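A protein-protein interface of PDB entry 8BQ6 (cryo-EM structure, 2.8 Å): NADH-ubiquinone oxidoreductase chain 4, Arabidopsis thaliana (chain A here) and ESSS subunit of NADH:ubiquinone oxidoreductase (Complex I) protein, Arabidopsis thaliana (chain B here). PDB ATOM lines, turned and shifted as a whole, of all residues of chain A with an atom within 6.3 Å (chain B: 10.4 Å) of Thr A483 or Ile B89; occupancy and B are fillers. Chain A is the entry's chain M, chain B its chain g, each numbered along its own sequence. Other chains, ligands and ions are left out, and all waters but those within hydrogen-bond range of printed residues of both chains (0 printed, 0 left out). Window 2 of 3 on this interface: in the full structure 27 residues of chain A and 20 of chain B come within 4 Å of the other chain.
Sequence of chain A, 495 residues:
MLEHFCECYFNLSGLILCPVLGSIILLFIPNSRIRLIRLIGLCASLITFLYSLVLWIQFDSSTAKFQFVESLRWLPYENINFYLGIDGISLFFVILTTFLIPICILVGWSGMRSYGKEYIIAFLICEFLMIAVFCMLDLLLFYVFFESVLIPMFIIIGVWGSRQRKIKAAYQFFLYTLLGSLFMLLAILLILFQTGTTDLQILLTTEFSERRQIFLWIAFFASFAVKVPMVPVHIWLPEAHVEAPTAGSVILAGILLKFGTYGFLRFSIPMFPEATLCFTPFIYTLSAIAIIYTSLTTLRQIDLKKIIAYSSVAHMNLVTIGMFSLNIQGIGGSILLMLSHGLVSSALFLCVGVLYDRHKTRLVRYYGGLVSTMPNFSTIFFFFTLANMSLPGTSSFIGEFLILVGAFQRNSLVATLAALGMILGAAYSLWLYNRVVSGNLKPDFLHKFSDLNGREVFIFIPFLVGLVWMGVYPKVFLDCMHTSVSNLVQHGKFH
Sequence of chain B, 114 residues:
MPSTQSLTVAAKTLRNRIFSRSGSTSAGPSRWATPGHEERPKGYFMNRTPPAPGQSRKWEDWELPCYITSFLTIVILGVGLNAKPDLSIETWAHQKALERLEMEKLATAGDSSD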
ATOM      1  N   SER A  61     -10.875  32.222 -25.711  1.00  0.00           N
ATOM      2  CA  SER A  61     -10.268  30.904 -25.601  1.00  0.00           C
ATOM      3  C   SER A  61     -11.185  29.782 -26.082  1.00  0.00           C
ATOM      4  O   SER A  61     -10.858  28.604 -25.904  1.00  0.00           O
ATOM      5  CB  SER A  61      -9.820  30.667 -24.158  1.00  0.00           C
ATOM      6  OG  SER A  61     -10.930  30.517 -23.295  1.00  0.00           O
ATOM      7  N   SER A  62     -12.315  30.124 -26.702  1.00  0.00           N
ATOM      8  CA  SER A  62     -13.207  29.141 -27.293  1.00  0.00           C
ATOM      9  C   SER A  62     -13.024  28.972 -28.792  1.00  0.00           C
ATOM     10  O   SER A  62     -13.556  28.011 -29.354  1.00  0.00           O
ATOM     11  CB  SER A  62     -14.669  29.517 -27.022  1.00  0.00           C
ATOM     12  OG  SER A  62     -15.035  30.676 -27.749  1.00  0.00           O
ATOM     13  N   THR A  63     -12.302  29.867 -29.448  1.00  0.00           N
ATOM     14  CA  THR A  63     -12.200  29.818 -30.895  1.00  0.00           C
ATOM     15  C   THR A  63     -10.874  29.204 -31.314  1.00  0.00           C
ATOM     16  O   THR A  63      -9.845  29.383 -30.657  1.00  0.00           O
ATOM     17  CB  THR A  63     -12.327  31.213 -31.509  1.00  0.00           C
ATOM     18  OG1 THR A  63     -12.034  31.145 -32.908  1.00  0.00           O
ATOM     19  CG2 THR A  63     -11.342  32.165 -30.869  1.00  0.00           C
ATOM     20  N   ALA A  64     -10.911  28.460 -32.410  1.00  0.00           N
ATOM     21  CA  ALA A  64      -9.682  28.027 -33.048  1.00  0.00           C
ATOM     22  C   ALA A  64      -9.260  28.947 -34.179  1.00  0.00           C
ATOM     23  O   ALA A  64      -8.198  28.730 -34.771  1.00  0.00           O
ATOM     24  CB  ALA A  64      -9.826  26.607 -33.578  1.00  0.00           C
ATOM     25  N   LEU A 478      -2.884  27.093 -19.646  1.00  0.00           N
ATOM     26  CA  LEU A 478      -3.384  25.970 -20.434  1.00  0.00           C
ATOM     27  C   LEU A 478      -4.803  26.208 -20.933  1.00  0.00           C
ATOM     28  O   LEU A 478      -5.144  25.780 -22.041  1.00  0.00           O
ATOM     29  CB  LEU A 478      -3.312  24.684 -19.616  1.00  0.00           C
ATOM     30  CG  LEU A 478      -1.910  24.104 -19.449  1.00  0.00           C
ATOM     31  CD1 LEU A 478      -1.933  22.943 -18.486  1.00  0.00           C
ATOM     32  CD2 LEU A 478      -1.381  23.662 -20.794  1.00  0.00           C
ATOM     33  N   ASP A 479      -5.635  26.891 -20.145  1.00  0.00           N
ATOM     34  CA  ASP A 479      -7.008  27.157 -20.564  1.00  0.00           C
ATOM     35  C   ASP A 479      -7.054  27.987 -21.839  1.00  0.00           C
ATOM     36  O   ASP A 479      -7.882  27.735 -22.723  1.00  0.00           O
ATOM     37  CB  ASP A 479      -7.766  27.876 -19.454  1.00  0.00           C
ATOM     38  CG  ASP A 479      -8.353  26.926 -18.441  1.00  0.00           C
ATOM     39  OD1 ASP A 479      -8.292  25.697 -18.659  1.00  0.00           O
ATOM     40  OD2 ASP A 479      -8.879  27.415 -17.422  1.00  0.00           O
ATOM     41  N   CYS A 480      -6.189  28.992 -21.945  1.00  0.00           N
ATOM     42  CA  CYS A 480      -6.185  29.865 -23.109  1.00  0.00           C
ATOM     43  C   CYS A 480      -5.533  29.226 -24.323  1.00  0.00           C
ATOM     44  O   CYS A 480      -5.546  29.828 -25.401  1.00  0.00           O
ATOM     45  CB  CYS A 480      -5.473  31.179 -22.781  1.00  0.00           C
ATOM     46  SG  CYS A 480      -6.340  32.231 -21.593  1.00  0.00           S
ATOM     47  N   MET A 481      -4.965  28.033 -24.173  1.00  0.00           N
ATOM     48  CA  MET A 481      -4.214  27.383 -25.236  1.00  0.00           C
ATOM     49  C   MET A 481      -4.911  26.173 -25.836  1.00  0.00           C
ATOM     50  O   MET A 481      -4.699  25.884 -27.015  1.00  0.00           O
ATOM     51  CB  MET A 481      -2.840  26.945 -24.711  1.00  0.00           C
ATOM     52  CG  MET A 481      -1.882  28.095 -24.467  1.00  0.00           C
ATOM     53  SD  MET A 481      -0.523  27.690 -23.357  1.00  0.00           S
ATOM     54  CE  MET A 481      -0.052  26.082 -23.981  1.00  0.00           C
ATOM     55  N   HIS A 482      -5.758  25.484 -25.068  1.00  0.00           N
ATOM     56  CA  HIS A 482      -6.164  24.130 -25.434  1.00  0.00           C
ATOM     57  C   HIS A 482      -6.967  24.088 -26.727  1.00  0.00           C
ATOM     58  O   HIS A 482      -6.943  23.081 -27.442  1.00  0.00           O
ATOM     59  CB  HIS A 482      -6.963  23.495 -24.299  1.00  0.00           C
ATOM     60  CG  HIS A 482      -6.108  22.816 -23.278  1.00  0.00           C
ATOM     61  ND1 HIS A 482      -6.504  22.644 -21.970  1.00  0.00           N
ATOM     62  CD2 HIS A 482      -4.865  22.289 -23.369  1.00  0.00           C
ATOM     63  CE1 HIS A 482      -5.548  22.024 -21.302  1.00  0.00           C
ATOM     64  NE2 HIS A 482      -4.542  21.798 -22.128  1.00  0.00           N
ATOM     65  N   THR A 483      -7.699  25.157 -27.040  1.00  0.00           N
ATOM     66  CA  THR A 483      -8.503  25.150 -28.259  1.00  0.00           C
ATOM     67  C   THR A 483      -7.620  25.238 -29.497  1.00  0.00           C
ATOM     68  O   THR A 483      -7.869  24.564 -30.503  1.00  0.00           O
ATOM     69  CB  THR A 483      -9.511  26.296 -28.239  1.00  0.00           C
ATOM     70  OG1 THR A 483     -10.236  26.273 -27.005  1.00  0.00           O
ATOM     71  CG2 THR A 483     -10.487  26.145 -29.389  1.00  0.00           C
ATOM     72  N   SER A 484      -6.588  26.083 -29.442  1.00  0.00           N
ATOM     73  CA  SER A 484      -5.622  26.164 -30.534  1.00  0.00           C
ATOM     74  C   SER A 484      -4.758  24.913 -30.595  1.00  0.00           C
ATOM     75  O   SER A 484      -4.407  24.437 -31.681  1.00  0.00           O
ATOM     76  CB  SER A 484      -4.748  27.404 -30.363  1.00  0.00           C
ATOM     77  OG  SER A 484      -5.511  28.588 -30.484  1.00  0.00           O
ATOM     78  N   VAL A 485      -4.376  24.385 -29.432  1.00  0.00           N
ATOM     79  CA  VAL A 485      -3.587  23.157 -29.401  1.00  0.00           C
ATOM     80  C   VAL A 485      -4.389  22.001 -29.979  1.00  0.00           C
ATOM     81  O   VAL A 485      -3.866  21.190 -30.753  1.00  0.00           O
ATOM     82  CB  VAL A 485      -3.115  22.859 -27.966  1.00  0.00           C
ATOM     83  CG1 VAL A 485      -2.665  21.410 -27.845  1.00  0.00           C
ATOM     84  CG2 VAL A 485      -1.993  23.797 -27.574  1.00  0.00           C
ATOM     85  N   SER A 486      -5.672  21.913 -29.625  1.00  0.00           N
ATOM     86  CA  SER A 486      -6.493  20.800 -30.086  1.00  0.00           C
ATOM     87  C   SER A 486      -6.618  20.796 -31.601  1.00  0.00           C
ATOM     88  O   SER A 486      -6.517  19.743 -32.239  1.00  0.00           O
ATOM     89  CB  SER A 486      -7.872  20.871 -29.440  1.00  0.00           C
ATOM     90  OG  SER A 486      -7.786  20.586 -28.059  1.00  0.00           O
ATOM     91  N   ASN A 487      -6.827  21.970 -32.193  1.00  0.00           N
ATOM     92  CA  ASN A 487      -7.003  22.055 -33.635  1.00  0.00           C
ATOM     93  C   ASN A 487      -5.685  21.886 -34.372  1.00  0.00           C
ATOM     94  O   ASN A 487      -5.674  21.459 -35.532  1.00  0.00           O
ATOM     95  CB  ASN A 487      -7.662  23.384 -33.984  1.00  0.00           C
ATOM     96  CG  ASN A 487      -9.167  23.298 -33.951  1.00  0.00           C
ATOM     97  OD1 ASN A 487      -9.796  23.610 -32.944  1.00  0.00           O
ATOM     98  ND2 ASN A 487      -9.756  22.875 -35.055  1.00  0.00           N
ATOM     99  N   LEU A 488      -4.569  22.181 -33.710  1.00  0.00           N
ATOM    100  CA  LEU A 488      -3.245  21.935 -34.338  1.00  0.00           C
ATOM    101  C   LEU A 488      -3.027  20.426 -34.428  1.00  0.00           C
ATOM    102  O   LEU A 488      -2.512  19.965 -35.460  1.00  0.00           O
ATOM    103  CB  LEU A 488      -2.160  22.611 -33.493  1.00  0.00           C
ATOM    104  CG  LEU A 488      -0.716  22.214 -33.782  1.00  0.00           C
ATOM    105  CD1 LEU A 488      -0.269  22.762 -35.124  1.00  0.00           C
ATOM    106  CD2 LEU A 488       0.192  22.723 -32.681  1.00  0.00           C
ATOM    107  N   PRO B  85     -14.904  36.353 -19.153  1.00  0.00           N
ATOM    108  CA  PRO B  85     -15.776  35.179 -19.083  1.00  0.00           C
ATOM    109  C   PRO B  85     -14.990  33.892 -19.286  1.00  0.00           C
ATOM    110  O   PRO B  85     -13.939  33.871 -19.928  1.00  0.00           O
ATOM    111  CB  PRO B  85     -16.777  35.413 -20.218  1.00  0.00           C
ATOM    112  CG  PRO B  85     -16.047  36.302 -21.178  1.00  0.00           C
ATOM    113  CD  PRO B  85     -15.200  37.196 -20.325  1.00  0.00           C
ATOM    114  N   ASP B  86     -15.506  32.811 -18.709  1.00  0.00           N
ATOM    115  CA  ASP B  86     -14.916  31.493 -18.907  1.00  0.00           C
ATOM    116  C   ASP B  86     -15.376  30.963 -20.258  1.00  0.00           C
ATOM    117  O   ASP B  86     -16.527  30.540 -20.407  1.00  0.00           O
ATOM    118  CB  ASP B  86     -15.316  30.552 -17.775  1.00  0.00           C
ATOM    119  CG  ASP B  86     -14.543  29.246 -17.796  1.00  0.00           C
ATOM    120  OD1 ASP B  86     -14.494  28.574 -16.747  1.00  0.00           O
ATOM    121  OD2 ASP B  86     -13.986  28.885 -18.854  1.00  0.00           O
ATOM    122  N   LEU B  87     -14.482  30.986 -21.244  1.00  0.00           N
ATOM    123  CA  LEU B  87     -14.780  30.475 -22.576  1.00  0.00           C
ATOM    124  C   LEU B  87     -13.890  29.302 -22.963  1.00  0.00           C
ATOM    125  O   LEU B  87     -13.616  29.105 -24.148  1.00  0.00           O
ATOM    126  CB  LEU B  87     -14.664  31.583 -23.621  1.00  0.00           C
ATOM    127  CG  LEU B  87     -15.317  32.935 -23.342  1.00  0.00           C
ATOM    128  CD1 LEU B  87     -14.673  34.001 -24.194  1.00  0.00           C
ATOM    129  CD2 LEU B  87     -16.798  32.873 -23.633  1.00  0.00           C
ATOM    130  N   SER B  88     -13.429  28.518 -21.995  1.00  0.00           N
ATOM    131  CA  SER B  88     -12.595  27.374 -22.326  1.00  0.00           C
ATOM    132  C   SER B  88     -13.426  26.287 -22.999  1.00  0.00           C
ATOM    133  O   SER B  88     -14.625  26.140 -22.747  1.00  0.00           O
ATOM    134  CB  SER B  88     -11.911  26.831 -21.071  1.00  0.00           C
ATOM    135  OG  SER B  88     -12.840  26.226 -20.192  1.00  0.00           O
ATOM    136  N   ILE B  89     -12.773  25.534 -23.889  1.00  0.00           N
ATOM    137  CA  ILE B  89     -13.419  24.388 -24.521  1.00  0.00           C
ATOM    138  C   ILE B  89     -13.808  23.360 -23.468  1.00  0.00           C
ATOM    139  O   ILE B  89     -14.766  22.599 -23.651  1.00  0.00           O
ATOM    140  CB  ILE B  89     -12.488  23.790 -25.596  1.00  0.00           C
ATOM    141  CG1 ILE B  89     -13.212  22.723 -26.416  1.00  0.00           C
ATOM    142  CG2 ILE B  89     -11.236  23.203 -24.965  1.00  0.00           C
ATOM    143  CD1 ILE B  89     -14.247  23.281 -27.356  1.00  0.00           C
ATOM    144  N   GLU B  90     -13.086  23.333 -22.346  1.00  0.00           N
ATOM    145  CA  GLU B  90     -13.397  22.398 -21.272  1.00  0.00           C
ATOM    146  C   GLU B  90     -14.713  22.751 -20.586  1.00  0.00           C
ATOM    147  O   GLU B  90     -15.517  21.866 -20.274  1.00  0.00           O
ATOM    148  CB  GLU B  90     -12.248  22.368 -20.265  1.00  0.00           C
ATOM    149  CG  GLU B  90     -10.872  22.394 -20.909  1.00  0.00           C
ATOM    150  CD  GLU B  90      -9.774  22.759 -19.932  1.00  0.00           C
ATOM    151  OE1 GLU B  90      -8.780  23.379 -20.364  1.00  0.00           O
ATOM    152  OE2 GLU B  90      -9.901  22.425 -18.735  1.00  0.00           O
ATOM    153  N   THR B  91     -14.949  24.038 -20.327  1.00  0.00           N
ATOM    154  CA  THR B  91     -16.183  24.414 -19.641  1.00  0.00           C
ATOM    155  C   THR B  91     -17.394  24.216 -20.542  1.00  0.00           C
ATOM    156  O   THR B  91     -18.467  23.818 -20.074  1.00  0.00           O
ATOM    157  CB  THR B  91     -16.101  25.858 -19.149  1.00  0.00           C
ATOM    158  OG1 THR B  91     -15.019  25.981 -18.219  1.00  0.00           O
ATOM    159  CG2 THR B  91     -17.390  26.265 -18.458  1.00  0.00           C
ATOM    160  N   TRP B  92     -17.236  24.476 -21.838  1.00  0.00           N
ATOM    161  CA  TRP B  92     -18.347  24.317 -22.766  1.00  0.00           C
ATOM    162  C   TRP B  92     -18.673  22.846 -22.991  1.00  0.00           C
ATOM    163  O   TRP B  92     -19.848  22.462 -23.024  1.00  0.00           O
ATOM    164  CB  TRP B  92     -18.015  25.008 -24.084  1.00  0.00           C
ATOM    165  CG  TRP B  92     -18.963  24.696 -25.176  1.00  0.00           C
ATOM    166  CD1 TRP B  92     -20.097  25.376 -25.482  1.00  0.00           C
ATOM    167  CD2 TRP B  92     -18.858  23.634 -26.130  1.00  0.00           C
ATOM    168  NE1 TRP B  92     -20.716  24.801 -26.563  1.00  0.00           N
ATOM    169  CE2 TRP B  92     -19.974  23.729 -26.980  1.00  0.00           C
ATOM    170  CE3 TRP B  92     -17.932  22.609 -26.344  1.00  0.00           C
ATOM    171  CZ2 TRP B  92     -20.191  22.840 -28.027  1.00  0.00           C
ATOM    172  CZ3 TRP B  92     -18.149  21.730 -27.385  1.00  0.00           C
ATOM    173  CH2 TRP B  92     -19.269  21.851 -28.214  1.00  0.00           C
ATOM    174  N   ALA B  93     -17.647  22.010 -23.147  1.00  0.00           N
ATOM    175  CA  ALA B  93     -17.887  20.589 -23.362  1.00  0.00           C
ATOM    176  C   ALA B  93     -18.426  19.910 -22.111  1.00  0.00           C
ATOM    177  O   ALA B  93     -19.186  18.942 -22.217  1.00  0.00           O
ATOM    178  CB  ALA B  93     -16.605  19.902 -23.826  1.00  0.00           C
ATOM    179  N   HIS B  94     -18.001  20.379 -20.932  1.00  0.00           N
ATOM    180  CA  HIS B  94     -18.511  19.805 -19.659  1.00  0.00           C
ATOM    181  C   HIS B  94     -20.029  19.930 -19.638  1.00  0.00           C
ATOM    182  O   HIS B  94     -20.702  18.905 -19.428  1.00  0.00           O
ATOM    183  CB  HIS B  94     -17.905  20.511 -18.443  1.00  0.00           C
ATOM    184  CG  HIS B  94     -18.295  19.881 -17.150  1.00  0.00           C
ATOM    185  ND1 HIS B  94     -18.020  18.560 -16.861  1.00  0.00           N
ATOM    186  CD2 HIS B  94     -18.950  20.376 -16.078  1.00  0.00           C
ATOM    187  CE1 HIS B  94     -18.480  18.270 -15.662  1.00  0.00           C
ATOM    188  NE2 HIS B  94     -19.055  19.368 -15.160  1.00  0.00           N
ATOM    189  N   GLN B  95     -20.534  21.146 -19.846  1.00  0.00           N
ATOM    190  CA  GLN B  95     -21.973  21.374 -19.876  1.00  0.00           C
ATOM    191  C   GLN B  95     -22.636  20.558 -20.979  1.00  0.00           C
ATOM    192  O   GLN B  95     -23.711  19.982 -20.776  1.00  0.00           O
ATOM    193  CB  GLN B  95     -22.248  22.861 -20.069  1.00  0.00           C
ATOM    194  CG  GLN B  95     -23.536  23.155 -20.784  1.00  0.00           C
ATOM    195  CD  GLN B  95     -24.615  23.583 -19.830  1.00  0.00           C
ATOM    196  OE1 GLN B  95     -24.465  23.461 -18.614  1.00  0.00           O
ATOM    197  NE2 GLN B  95     -25.713  24.091 -20.369  1.00  0.00           N
ATOM    198  N   LYS B  96     -22.007  20.508 -22.153  1.00  0.00           N
ATOM    199  CA  LYS B  96     -22.555  19.748 -23.271  1.00  0.00           C
ATOM    200  C   LYS B  96     -22.598  18.258 -22.962  1.00  0.00           C
ATOM    201  O   LYS B  96     -23.552  17.568 -23.336  1.00  0.00           O
ATOM    202  CB  LYS B  96     -21.724  20.004 -24.525  1.00  0.00           C
ATOM    203  CG  LYS B  96     -22.160  21.211 -25.311  1.00  0.00           C
ATOM    204  CD  LYS B  96     -23.313  20.883 -26.226  1.00  0.00           C
ATOM    205  CE  LYS B  96     -24.019  22.151 -26.659  1.00  0.00           C
ATOM    206  NZ  LYS B  96     -24.087  23.126 -25.537  1.00  0.00           N
ATOM    207  N   ALA B  97     -21.565  17.742 -22.294  1.00  0.00           N
ATOM    208  CA  ALA B  97     -21.511  16.313 -22.009  1.00  0.00           C
ATOM    209  C   ALA B  97     -22.489  15.935 -20.903  1.00  0.00           C
ATOM    210  O   ALA B  97     -22.960  14.793 -20.843  1.00  0.00           O
ATOM    211  CB  ALA B  97     -20.086  15.905 -21.635  1.00  0.00           C
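The backbone carbonyl oxygen (O) of Leu B87 is in hydrogen-bond range of the side-chain hydroxyl (OG) of Ser A61.
OG of Ser A61 lies within hydrogen-bond range of N of Ser B88, 3.5 Å away.
O of Leu B87 lies within hydrogen-bond range of N of Ser A62, at 3.0 Å.
A ring nitrogen (ND1) of His A482 is in hydrogen-bond range of the side-chain carboxylate (OE1) of Glu B90, 2.9 Å away.
The side-chain carboxylate of Asp A479 lies close to the side-chain carboxylate of Glu B90 (2.9 Å).
Hydrophobic or aromatic side chains of chain A within 4 Å of the printed part of chain B: His A482.
Hydrophobic or aromatic side chains of chain B within 4 Å of the printed part of chain A: Leu B87 and Ile B89.
Among the printed residues, 6 pairs touch across the chains.
Among the printed residues, no Asp or Glu carboxylate lies within 4 Å of a Lys or Arg side-chain nitrogen of the other chain.
Among the printed residues, merely in contact across the chains: Thr A483 with Ile B89 (3.6 Å).
Of chain A, only Thr A483 (3.6 Å) comes within 4 Å of Ile B89.
Ser A61 touches just these residues of chain B: Leu B87 (3.2 Å) and Ser B88 (3.5 Å).
Thr A63 touches none of the printed residues of chain B.
No residue of chain B comes within 4 Å of Ala A64.
No residue of chain B comes within 4 Å of Val A485.
No residue of chain B comes within 4 Å of Ser A486.
No residue of chain B comes within 4 Å of Asn A487.
Of the printed residues of chain A, Leu B87 touches Ser A61 (3.2 Å) and Ser A62 (3.0 Å).
Printed residues of chain A within 4 Å of Glu B90: Asp A479 and His A482.
His B94 touches none of the printed residues of chain A.
Leu A488 touches none of the printed residues of chain B.
The nearest residue of chain B that does not touch Thr A483 is Ser B88 (5.1 Å).
The side-chain hydroxyl of Thr A483 sits at hydrogen-bond distance from the backbone carbonyl oxygen of Ser A61, 2.7 Å away.
ND1 of His A482 sits close to O of Leu A478 (3.4 Å).
OG of Ser A486 sits at hydrogen-bond distance from O of His A482, at 2.7 Å.
O of Thr A483 lies close to OD1 of Asn A487 (3.3 Å).
OD2 of Asp B86 is in hydrogen-bond range of OG of Ser B88 (3.2 Å).
The side-chain hydroxyl of Thr B91 is in hydrogen-bond range of the side-chain hydroxyl of Ser B88 (2.9 Å).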
